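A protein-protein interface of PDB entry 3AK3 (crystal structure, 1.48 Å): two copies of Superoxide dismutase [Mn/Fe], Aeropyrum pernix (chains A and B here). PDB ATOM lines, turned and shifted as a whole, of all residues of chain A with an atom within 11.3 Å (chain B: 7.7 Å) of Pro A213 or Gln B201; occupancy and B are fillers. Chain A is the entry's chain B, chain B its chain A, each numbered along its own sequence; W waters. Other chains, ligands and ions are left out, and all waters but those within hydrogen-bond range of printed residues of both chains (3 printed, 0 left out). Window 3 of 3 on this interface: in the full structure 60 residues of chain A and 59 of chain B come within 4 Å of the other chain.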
ATOM      1  N   PRO A 137      -5.900   1.667  14.091  1.00  0.00           N
ATOM      2  CA  PRO A 137      -6.609   0.957  13.017  1.00  0.00           C
ATOM      3  C   PRO A 137      -5.713   0.133  12.091  1.00  0.00           C
ATOM      4  O   PRO A 137      -6.202  -0.799  11.459  1.00  0.00           O
ATOM      5  CB  PRO A 137      -7.265   2.088  12.227  1.00  0.00           C
ATOM      6  CG  PRO A 137      -6.373   3.275  12.483  1.00  0.00           C
ATOM      7  CD  PRO A 137      -5.979   3.129  13.927  1.00  0.00           C
ATOM      8  N   GLU A 140      -4.819  -2.940  14.741  1.00  0.00           N
ATOM      9  CA  GLU A 140      -5.883  -3.348  15.657  1.00  0.00           C
ATOM     10  C   GLU A 140      -5.320  -3.684  17.038  1.00  0.00           C
ATOM     11  O   GLU A 140      -5.713  -4.665  17.676  1.00  0.00           O
ATOM     12  CB  GLU A 140      -6.716  -4.482  15.044  1.00  0.00           C
ATOM     13  CG  GLU A 140      -7.424  -4.038  13.761  1.00  0.00           C
ATOM     14  CD  GLU A 140      -8.556  -4.952  13.350  1.00  0.00           C
ATOM     15  OE1 GLU A 140      -9.713  -4.478  13.300  1.00  0.00           O
ATOM     16  OE2 GLU A 140      -8.288  -6.134  13.065  1.00  0.00           O
ATOM     17  N   GLN A 201     -16.508  -0.693  19.480  1.00  0.00           N
ATOM     18  CA  GLN A 201     -16.769   0.094  18.281  1.00  0.00           C
ATOM     19  C   GLN A 201     -15.540   0.190  17.394  1.00  0.00           C
ATOM     20  O   GLN A 201     -15.647   0.045  16.181  1.00  0.00           O
ATOM     21  CB  GLN A 201     -17.310   1.484  18.625  1.00  0.00           C
ATOM     22  CG  GLN A 201     -18.695   1.462  19.278  1.00  0.00           C
ATOM     23  CD  GLN A 201     -19.717   0.659  18.485  1.00  0.00           C
ATOM     24  OE1 GLN A 201     -20.417  -0.190  19.041  1.00  0.00           O
ATOM     25  NE2 GLN A 201     -19.801   0.916  17.183  1.00  0.00           N
ATOM     26  N   ALA A 202     -14.375   0.398  18.005  1.00  0.00           N
ATOM     27  CA  ALA A 202     -13.126   0.498  17.254  1.00  0.00           C
ATOM     28  C   ALA A 202     -12.783  -0.798  16.512  1.00  0.00           C
ATOM     29  O   ALA A 202     -12.448  -0.770  15.329  1.00  0.00           O
ATOM     30  CB  ALA A 202     -11.991   0.927  18.169  1.00  0.00           C
ATOM     31  N   LEU A 203     -12.892  -1.931  17.200  1.00  0.00           N
ATOM     32  CA  LEU A 203     -12.628  -3.240  16.603  1.00  0.00           C
ATOM     33  C   LEU A 203     -13.499  -3.498  15.377  1.00  0.00           C
ATOM     34  O   LEU A 203     -13.062  -4.119  14.408  1.00  0.00           O
ATOM     35  CB  LEU A 203     -12.844  -4.342  17.643  1.00  0.00           C
ATOM     36  CG  LEU A 203     -11.708  -4.469  18.662  1.00  0.00           C
ATOM     37  CD1 LEU A 203     -12.177  -5.144  19.940  1.00  0.00           C
ATOM     38  CD2 LEU A 203     -10.520  -5.205  18.052  1.00  0.00           C
ATOM     39  N   ASN A 204     -14.726  -2.990  15.421  1.00  0.00           N
ATOM     40  CA  ASN A 204     -15.677  -3.183  14.337  1.00  0.00           C
ATOM     41  C   ASN A 204     -15.530  -2.193  13.184  1.00  0.00           C
ATOM     42  O   ASN A 204     -15.777  -2.547  12.024  1.00  0.00           O
ATOM     43  CB  ASN A 204     -17.104  -3.145  14.884  1.00  0.00           C
ATOM     44  CG  ASN A 204     -17.470  -4.412  15.615  1.00  0.00           C
ATOM     45  OD1 ASN A 204     -16.985  -5.490  15.276  1.00  0.00           O
ATOM     46  ND2 ASN A 204     -18.329  -4.294  16.624  1.00  0.00           N
ATOM     47  N   ASN A 205     -15.106  -0.968  13.507  1.00  0.00           N
ATOM     48  CA  ASN A 205     -15.260   0.175  12.602  1.00  0.00           C
ATOM     49  C   ASN A 205     -13.990   0.902  12.150  1.00  0.00           C
ATOM     50  O   ASN A 205     -13.997   1.528  11.094  1.00  0.00           O
ATOM     51  CB  ASN A 205     -16.197   1.214  13.224  1.00  0.00           C
ATOM     52  CG  ASN A 205     -17.629   0.730  13.325  1.00  0.00           C
ATOM     53  OD1 ASN A 205     -17.912  -0.308  13.919  1.00  0.00           O
ATOM     54  ND2 ASN A 205     -18.543   1.491  12.753  1.00  0.00           N
ATOM     55  N   ALA A 206     -12.919   0.839  12.939  1.00  0.00           N
ATOM     56  CA  ALA A 206     -11.770   1.727  12.709  1.00  0.00           C
ATOM     57  C   ALA A 206     -10.913   1.347  11.493  1.00  0.00           C
ATOM     58  O   ALA A 206     -10.638   2.184  10.630  1.00  0.00           O
ATOM     59  CB  ALA A 206     -10.913   1.845  13.966  1.00  0.00           C
ATOM     60  N   LYS A 207     -10.485   0.093  11.419  1.00  0.00           N
ATOM     61  CA  LYS A 207      -9.573  -0.327  10.352  1.00  0.00           C
ATOM     62  C   LYS A 207     -10.038   0.041   8.918  1.00  0.00           C
ATOM     63  O   LYS A 207      -9.253   0.592   8.143  1.00  0.00           O
ATOM     64  CB  LYS A 207      -9.245  -1.820  10.484  1.00  0.00           C
ATOM     65  CG  LYS A 207      -8.262  -2.343   9.450  1.00  0.00           C
ATOM     66  CD  LYS A 207      -8.003  -3.813   9.685  1.00  0.00           C
ATOM     67  CE  LYS A 207      -7.065  -4.379   8.651  1.00  0.00           C
ATOM     68  NZ  LYS A 207      -6.837  -5.828   8.919  1.00  0.00           N
ATOM     69  N   PRO A 208     -11.313  -0.237   8.573  1.00  0.00           N
ATOM     70  CA  PRO A 208     -11.847   0.077   7.239  1.00  0.00           C
ATOM     71  C   PRO A 208     -11.802   1.556   6.812  1.00  0.00           C
ATOM     72  O   PRO A 208     -11.895   1.841   5.621  1.00  0.00           O
ATOM     73  CB  PRO A 208     -13.308  -0.382   7.329  1.00  0.00           C
ATOM     74  CG  PRO A 208     -13.341  -1.366   8.421  1.00  0.00           C
ATOM     75  CD  PRO A 208     -12.332  -0.894   9.411  1.00  0.00           C
ATOM     76  N   LEU A 209     -11.657   2.482   7.761  1.00  0.00           N
ATOM     77  CA  LEU A 209     -11.543   3.908   7.421  1.00  0.00           C
ATOM     78  C   LEU A 209     -10.270   4.234   6.642  1.00  0.00           C
ATOM     79  O   LEU A 209     -10.196   5.261   5.960  1.00  0.00           O
ATOM     80  CB  LEU A 209     -11.553   4.762   8.689  1.00  0.00           C
ATOM     81  CG  LEU A 209     -12.796   4.729   9.566  1.00  0.00           C
ATOM     82  CD1 LEU A 209     -12.515   5.405  10.888  1.00  0.00           C
ATOM     83  CD2 LEU A 209     -13.928   5.419   8.846  1.00  0.00           C
ATOM     84  N   TYR A 210      -9.284   3.349   6.749  1.00  0.00           N
ATOM     85  CA  TYR A 210      -7.925   3.628   6.298  1.00  0.00           C
ATOM     86  C   TYR A 210      -7.394   2.583   5.342  1.00  0.00           C
ATOM     87  O   TYR A 210      -6.717   2.908   4.356  1.00  0.00           O
ATOM     88  CB  TYR A 210      -7.009   3.738   7.512  1.00  0.00           C
ATOM     89  CG  TYR A 210      -7.437   4.870   8.389  1.00  0.00           C
ATOM     90  CD1 TYR A 210      -7.224   6.187   7.986  1.00  0.00           C
ATOM     91  CD2 TYR A 210      -8.105   4.636   9.596  1.00  0.00           C
ATOM     92  CE1 TYR A 210      -7.630   7.242   8.761  1.00  0.00           C
ATOM     93  CE2 TYR A 210      -8.517   5.694  10.384  1.00  0.00           C
ATOM     94  CZ  TYR A 210      -8.276   6.997   9.955  1.00  0.00           C
ATOM     95  OH  TYR A 210      -8.661   8.076  10.709  1.00  0.00           O
ATOM     96  N   LEU A 211      -7.682   1.328   5.659  1.00  0.00           N
ATOM     97  CA  LEU A 211      -7.350   0.218   4.792  1.00  0.00           C
ATOM     98  C   LEU A 211      -8.680  -0.285   4.257  1.00  0.00           C
ATOM     99  O   LEU A 211      -9.437  -0.962   4.962  1.00  0.00           O
ATOM    100  CB  LEU A 211      -6.568  -0.860   5.556  1.00  0.00           C
ATOM    101  CG  LEU A 211      -5.314  -0.364   6.295  1.00  0.00           C
ATOM    102  CD1 LEU A 211      -4.655  -1.487   7.089  1.00  0.00           C
ATOM    103  CD2 LEU A 211      -4.311   0.298   5.347  1.00  0.00           C
ATOM    104  N   LEU A 212      -8.967   0.095   3.013  1.00  0.00           N
ATOM    105  CA  LEU A 212     -10.276  -0.128   2.387  1.00  0.00           C
ATOM    106  C   LEU A 212     -10.616  -1.612   2.219  1.00  0.00           C
ATOM    107  O   LEU A 212      -9.780  -2.384   1.747  1.00  0.00           O
ATOM    108  CB  LEU A 212     -10.354   0.604   1.037  1.00  0.00           C
ATOM    109  CG  LEU A 212     -10.182   2.135   1.038  1.00  0.00           C
ATOM    110  CD1 LEU A 212     -10.172   2.676  -0.378  1.00  0.00           C
ATOM    111  CD2 LEU A 212     -11.255   2.830   1.866  1.00  0.00           C
ATOM    112  N   PRO A 213     -11.849  -2.013   2.602  1.00  0.00           N
ATOM    113  CA  PRO A 213     -12.224  -3.426   2.581  1.00  0.00           C
ATOM    114  C   PRO A 213     -12.823  -3.864   1.244  1.00  0.00           C
ATOM    115  O   PRO A 213     -12.355  -3.437   0.189  1.00  0.00           O
ATOM    116  CB  PRO A 213     -13.275  -3.516   3.694  1.00  0.00           C
ATOM    117  CG  PRO A 213     -13.919  -2.150   3.720  1.00  0.00           C
ATOM    118  CD  PRO A 213     -12.962  -1.165   3.074  1.00  0.00           C
ATOM    119  N   PHE B 135     -13.263  13.859   7.295  1.00  0.00           N
ATOM    120  CA  PHE B 135     -14.643  13.641   7.689  1.00  0.00           C
ATOM    121  C   PHE B 135     -14.748  13.790   9.200  1.00  0.00           C
ATOM    122  O   PHE B 135     -13.982  13.189   9.943  1.00  0.00           O
ATOM    123  CB  PHE B 135     -15.094  12.249   7.259  1.00  0.00           C
ATOM    124  CG  PHE B 135     -16.537  11.946   7.553  1.00  0.00           C
ATOM    125  CD1 PHE B 135     -17.532  12.367   6.684  1.00  0.00           C
ATOM    126  CD2 PHE B 135     -16.898  11.219   8.686  1.00  0.00           C
ATOM    127  CE1 PHE B 135     -18.864  12.070   6.938  1.00  0.00           C
ATOM    128  CE2 PHE B 135     -18.231  10.921   8.944  1.00  0.00           C
ATOM    129  CZ  PHE B 135     -19.208  11.351   8.063  1.00  0.00           C
ATOM    130  N   VAL B 159     -11.248  12.186  10.317  1.00  0.00           N
ATOM    131  CA  VAL B 159     -10.719  11.129   9.464  1.00  0.00           C
ATOM    132  C   VAL B 159     -10.234  11.732   8.150  1.00  0.00           C
ATOM    133  O   VAL B 159     -11.065  12.154   7.350  1.00  0.00           O
ATOM    134  CB  VAL B 159     -11.821  10.087   9.156  1.00  0.00           C
ATOM    135  CG1 VAL B 159     -11.299   8.956   8.259  1.00  0.00           C
ATOM    136  CG2 VAL B 159     -12.418   9.551  10.455  1.00  0.00           C
ATOM    137  N   ILE B 161      -9.622  12.001   4.501  1.00  0.00           N
ATOM    138  CA  ILE B 161     -10.022  11.257   3.303  1.00  0.00           C
ATOM    139  C   ILE B 161      -9.232  11.681   2.051  1.00  0.00           C
ATOM    140  O   ILE B 161      -9.130  10.920   1.076  1.00  0.00           O
ATOM    141  CB  ILE B 161     -11.565  11.300   3.069  1.00  0.00           C
ATOM    142  CG1 ILE B 161     -12.051  12.724   2.745  1.00  0.00           C
ATOM    143  CG2 ILE B 161     -12.302  10.697   4.275  1.00  0.00           C
ATOM    144  CD1 ILE B 161     -13.479  12.782   2.186  1.00  0.00           C
ATOM    145  N   VAL B 195     -10.981   8.716  -2.883  1.00  0.00           N
ATOM    146  CA  VAL B 195     -11.591   9.630  -1.916  1.00  0.00           C
ATOM    147  C   VAL B 195     -13.042   9.248  -1.633  1.00  0.00           C
ATOM    148  O   VAL B 195     -13.474   9.244  -0.481  1.00  0.00           O
ATOM    149  CB  VAL B 195     -11.478  11.118  -2.355  1.00  0.00           C
ATOM    150  CG1 VAL B 195     -12.105  12.042  -1.320  1.00  0.00           C
ATOM    151  CG2 VAL B 195     -10.016  11.498  -2.575  1.00  0.00           C
ATOM    152  N   GLU B 196     -13.780   8.911  -2.690  1.00  0.00           N
ATOM    153  CA  GLU B 196     -15.175   8.503  -2.567  1.00  0.00           C
ATOM    154  C   GLU B 196     -15.295   7.253  -1.696  1.00  0.00           C
ATOM    155  O   GLU B 196     -16.174   7.166  -0.838  1.00  0.00           O
ATOM    156  CB  GLU B 196     -15.775   8.256  -3.958  1.00  0.00           C
ATOM    157  CG  GLU B 196     -17.242   7.807  -3.960  1.00  0.00           C
ATOM    158  CD  GLU B 196     -18.221   8.927  -3.653  1.00  0.00           C
ATOM    159  OE1 GLU B 196     -17.811  10.107  -3.612  1.00  0.00           O
ATOM    160  OE2 GLU B 196     -19.415   8.622  -3.459  1.00  0.00           O
ATOM    161  N   LYS B 197     -14.388   6.298  -1.903  1.00  0.00           N
ATOM    162  CA  LYS B 197     -14.409   5.050  -1.137  1.00  0.00           C
ATOM    163  C   LYS B 197     -14.078   5.295   0.337  1.00  0.00           C
ATOM    164  O   LYS B 197     -14.647   4.661   1.223  1.00  0.00           O
ATOM    165  CB  LYS B 197     -13.467   4.009  -1.748  1.00  0.00           C
ATOM    166  CG  LYS B 197     -13.965   3.427  -3.074  1.00  0.00           C
ATOM    167  CD  LYS B 197     -12.880   2.613  -3.773  1.00  0.00           C
ATOM    168  CE  LYS B 197     -13.464   1.658  -4.812  1.00  0.00           C
ATOM    169  NZ  LYS B 197     -14.171   2.348  -5.927  1.00  0.00           N
ATOM    170  N   ARG B 198     -13.163   6.225   0.591  1.00  0.00           N
ATOM    171  CA  ARG B 198     -12.849   6.614   1.961  1.00  0.00           C
ATOM    172  C   ARG B 198     -14.039   7.277   2.640  1.00  0.00           C
ATOM    173  O   ARG B 198     -14.377   6.947   3.784  1.00  0.00           O
ATOM    174  CB  ARG B 198     -11.621   7.526   2.006  1.00  0.00           C
ATOM    175  CG  ARG B 198     -10.364   6.755   1.743  1.00  0.00           C
ATOM    176  CD  ARG B 198      -9.111   7.617   1.681  1.00  0.00           C
ATOM    177  NE  ARG B 198      -8.089   6.791   1.062  1.00  0.00           N
ATOM    178  CZ  ARG B 198      -7.347   5.879   1.689  1.00  0.00           C
ATOM    179  NH1 ARG B 198      -7.438   5.716   3.008  1.00  0.00           N
ATOM    180  NH2 ARG B 198      -6.492   5.144   0.988  1.00  0.00           N
ATOM    181  N   LEU B 199     -14.678   8.203   1.930  1.00  0.00           N
ATOM    182  CA  LEU B 199     -15.842   8.882   2.470  1.00  0.00           C
ATOM    183  C   LEU B 199     -16.959   7.897   2.774  1.00  0.00           C
ATOM    184  O   LEU B 199     -17.633   8.020   3.797  1.00  0.00           O
ATOM    185  CB  LEU B 199     -16.336   9.960   1.513  1.00  0.00           C
ATOM    186  CG  LEU B 199     -17.636  10.656   1.921  1.00  0.00           C
ATOM    187  CD1 LEU B 199     -17.552  11.327   3.286  1.00  0.00           C
ATOM    188  CD2 LEU B 199     -18.048  11.651   0.875  1.00  0.00           C
ATOM    189  N   GLU B 200     -17.152   6.918   1.897  1.00  0.00           N
ATOM    190  CA  GLU B 200     -18.220   5.953   2.124  1.00  0.00           C
ATOM    191  C   GLU B 200     -17.974   5.141   3.402  1.00  0.00           C
ATOM    192  O   GLU B 200     -18.905   4.887   4.161  1.00  0.00           O
ATOM    193  CB  GLU B 200     -18.472   5.081   0.893  1.00  0.00           C
ATOM    194  CG  GLU B 200     -17.502   3.960   0.672  1.00  0.00           C
ATOM    195  CD  GLU B 200     -18.091   2.849  -0.173  1.00  0.00           C
ATOM    196  OE1 GLU B 200     -18.095   2.974  -1.419  1.00  0.00           O
ATOM    197  OE2 GLU B 200     -18.546   1.848   0.417  1.00  0.00           O
ATOM    198  N   GLN B 201     -16.715   4.782   3.664  1.00  0.00           N
ATOM    199  CA  GLN B 201     -16.385   4.074   4.896  1.00  0.00           C
ATOM    200  C   GLN B 201     -16.592   4.974   6.104  1.00  0.00           C
ATOM    201  O   GLN B 201     -17.118   4.530   7.119  1.00  0.00           O
ATOM    202  CB  GLN B 201     -14.952   3.528   4.873  1.00  0.00           C
ATOM    203  CG  GLN B 201     -14.728   2.407   3.849  1.00  0.00           C
ATOM    204  CD  GLN B 201     -15.607   1.180   4.104  1.00  0.00           C
ATOM    205  OE1 GLN B 201     -15.849   0.798   5.248  1.00  0.00           O
ATOM    206  NE2 GLN B 201     -16.095   0.571   3.031  1.00  0.00           N
ATOM    207  N   ALA B 202     -16.204   6.243   5.981  1.00  0.00           N
ATOM    208  CA  ALA B 202     -16.365   7.203   7.078  1.00  0.00           C
ATOM    209  C   ALA B 202     -17.838   7.466   7.410  1.00  0.00           C
ATOM    210  O   ALA B 202     -18.219   7.501   8.585  1.00  0.00           O
ATOM    211  CB  ALA B 202     -15.634   8.504   6.766  1.00  0.00           C
ATOM    212  N   LEU B 203     -18.655   7.635   6.375  1.00  0.00           N
ATOM    213  CA  LEU B 203     -20.097   7.795   6.552  1.00  0.00           C
ATOM    214  C   LEU B 203     -20.688   6.603   7.289  1.00  0.00           C
ATOM    215  O   LEU B 203     -21.579   6.762   8.121  1.00  0.00           O
ATOM    216  CB  LEU B 203     -20.791   7.956   5.200  1.00  0.00           C
ATOM    217  CG  LEU B 203     -20.656   9.303   4.490  1.00  0.00           C
ATOM    218  CD1 LEU B 203     -20.904   9.126   2.999  1.00  0.00           C
ATOM    219  CD2 LEU B 203     -21.601  10.337   5.080  1.00  0.00           C
ATOM    220  N   ASN B 204     -20.182   5.412   6.980  1.00  0.00           N
ATOM    221  CA  ASN B 204     -20.670   4.185   7.596  1.00  0.00           C
ATOM    222  C   ASN B 204     -20.144   3.992   9.003  1.00  0.00           C
ATOM    223  O   ASN B 204     -20.871   3.503   9.863  1.00  0.00           O
ATOM    224  CB  ASN B 204     -20.298   2.955   6.760  1.00  0.00           C
ATOM    225  CG  ASN B 204     -21.093   2.847   5.471  1.00  0.00           C
ATOM    226  OD1 ASN B 204     -20.725   2.087   4.574  1.00  0.00           O
ATOM    227  ND2 ASN B 204     -22.184   3.605   5.368  1.00  0.00           N
ATOM    228  N   ASN B 205     -18.890   4.384   9.241  1.00  0.00           N
ATOM    229  CA  ASN B 205     -18.154   3.905  10.419  1.00  0.00           C
ATOM    230  C   ASN B 205     -17.708   4.917  11.474  1.00  0.00           C
ATOM    231  O   ASN B 205     -17.544   4.555  12.636  1.00  0.00           O
ATOM    232  CB  ASN B 205     -16.925   3.091   9.980  1.00  0.00           C
ATOM    233  CG  ASN B 205     -17.289   1.728   9.415  1.00  0.00           C
ATOM    234  OD1 ASN B 205     -18.433   1.476   9.038  1.00  0.00           O
ATOM    235  ND2 ASN B 205     -16.310   0.844   9.351  1.00  0.00           N
ATOM    236  N   ALA B 206     -17.485   6.167  11.081  1.00  0.00           N
ATOM    237  CA  ALA B 206     -16.781   7.115  11.955  1.00  0.00           C
ATOM    238  C   ALA B 206     -17.537   7.536  13.229  1.00  0.00           C
ATOM    239  O   ALA B 206     -16.993   7.459  14.330  1.00  0.00           O
ATOM    240  CB  ALA B 206     -16.330   8.330  11.158  1.00  0.00           C
ATOM    241  N   LYS B 207     -18.786   7.969  13.083  1.00  0.00           N
ATOM    242  CA  LYS B 207     -19.547   8.508  14.226  1.00  0.00           C
ATOM    243  C   LYS B 207     -19.583   7.614  15.488  1.00  0.00           C
ATOM    244  O   LYS B 207     -19.273   8.098  16.579  1.00  0.00           O
ATOM    245  CB  LYS B 207     -20.957   8.950  13.800  1.00  0.00           C
ATOM    246  CG  LYS B 207     -21.767   9.597  14.923  1.00  0.00           C
ATOM    247  CD  LYS B 207     -22.899  10.453  14.393  1.00  0.00           C
ATOM    248  CE  LYS B 207     -23.531  11.256  15.521  1.00  0.00           C
ATOM    249  NZ  LYS B 207     -24.513  12.261  15.016  1.00  0.00           N
HETATM  250  O   HOH W   1      -8.748   7.468   5.000  1.00  0.00           O
HETATM  251  O   HOH W   2     -12.478   6.874   5.718  1.00  0.00           O
HETATM  252  O   HOH W   3     -17.040  -1.789   9.201  1.00  0.00           O
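The backbone carbonyl oxygen (O) of Val B159 lies within hydrogen-bond range of the backbone NH (N) of Phe B135, 2.8 Å away. The backbone carbonyl oxygen of Gln A201 sits close to the side-chain amide oxygen of Asn A205 (3.2 Å).
Among the printed residues, merely in contact across the chains: Pro A208 with Gln B201, Leu A209 with Ala B202, Pro A213 with Gln B201, Tyr A210 with Val B159, Leu A209 with Gln B201, Leu A212 with Lys B197, Pro A208 with Asn B205 and Leu A209 with Asn B205.
Asn A205 touches its own counterpart, Asn B205. 7 positions are printed for both chains.
O of Tyr A210 sits at hydrogen-bond distance from NH1 of Arg B198 (3.2 Å). The backbone carbonyl oxygen (O) of Asn A205 is in hydrogen-bond range of the side-chain amide nitrogen (ND2) of Asn B205 (3.0 Å).
Of the 15 printed residues of chain A, 6 touch a printed residue of chain B. Among the printed residues, 10 pairs touch across the chains. Among the printed residues, no Asp or Glu carboxylate lies within 4 Å of a Lys or Arg side-chain nitrogen of the other chain.
Of chain B, only Gln B201 (3.6 Å) comes within 4 Å of Pro A213. Gln B201 touches three residues of chain A. Glu B200 touches none of the printed residues of chain A. Ala B202 touches just one residue of chain A: Leu A209. No residue of chain A comes within 4 Å of Asn B204. Of the printed residues of chain A, Asn B205 touches Asn A205, Pro A208 and Leu A209. Of the printed residues of chain B, Leu A209 touches Gln B201, Ala B202 and Asn B205. Of the printed residues of chain B, Tyr A210 touches Val B159 (3.7 Å) and Arg B198 (3.2 Å). Printed residues of chain A within 4 Å of Lys B197: Leu A212. Ala A202 touches none of the printed residues of chain B. The nearest residue of chain B that does not touch Pro A213 is Lys B197 (6.3 Å). The nearest printed residue of chain A that does not touch Val B159 is Leu A209 (4.2 Å).
Water W2 lies within hydrogen-bond range of the backbone carbonyl oxygen (O) of Arg B198 (2.7 Å) and the backbone carbonyl oxygen (O) of Leu A209 (2.8 Å). Water W3 bridges the side-chain amide nitrogen (ND2) of Asn B205 and the backbone carbonyl oxygen (O) of Asn A204. Water W1 bridges the backbone carbonyl oxygen of Leu A209 (2.8 Å) and the guanidinium group of Arg B198 (3.0 Å).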
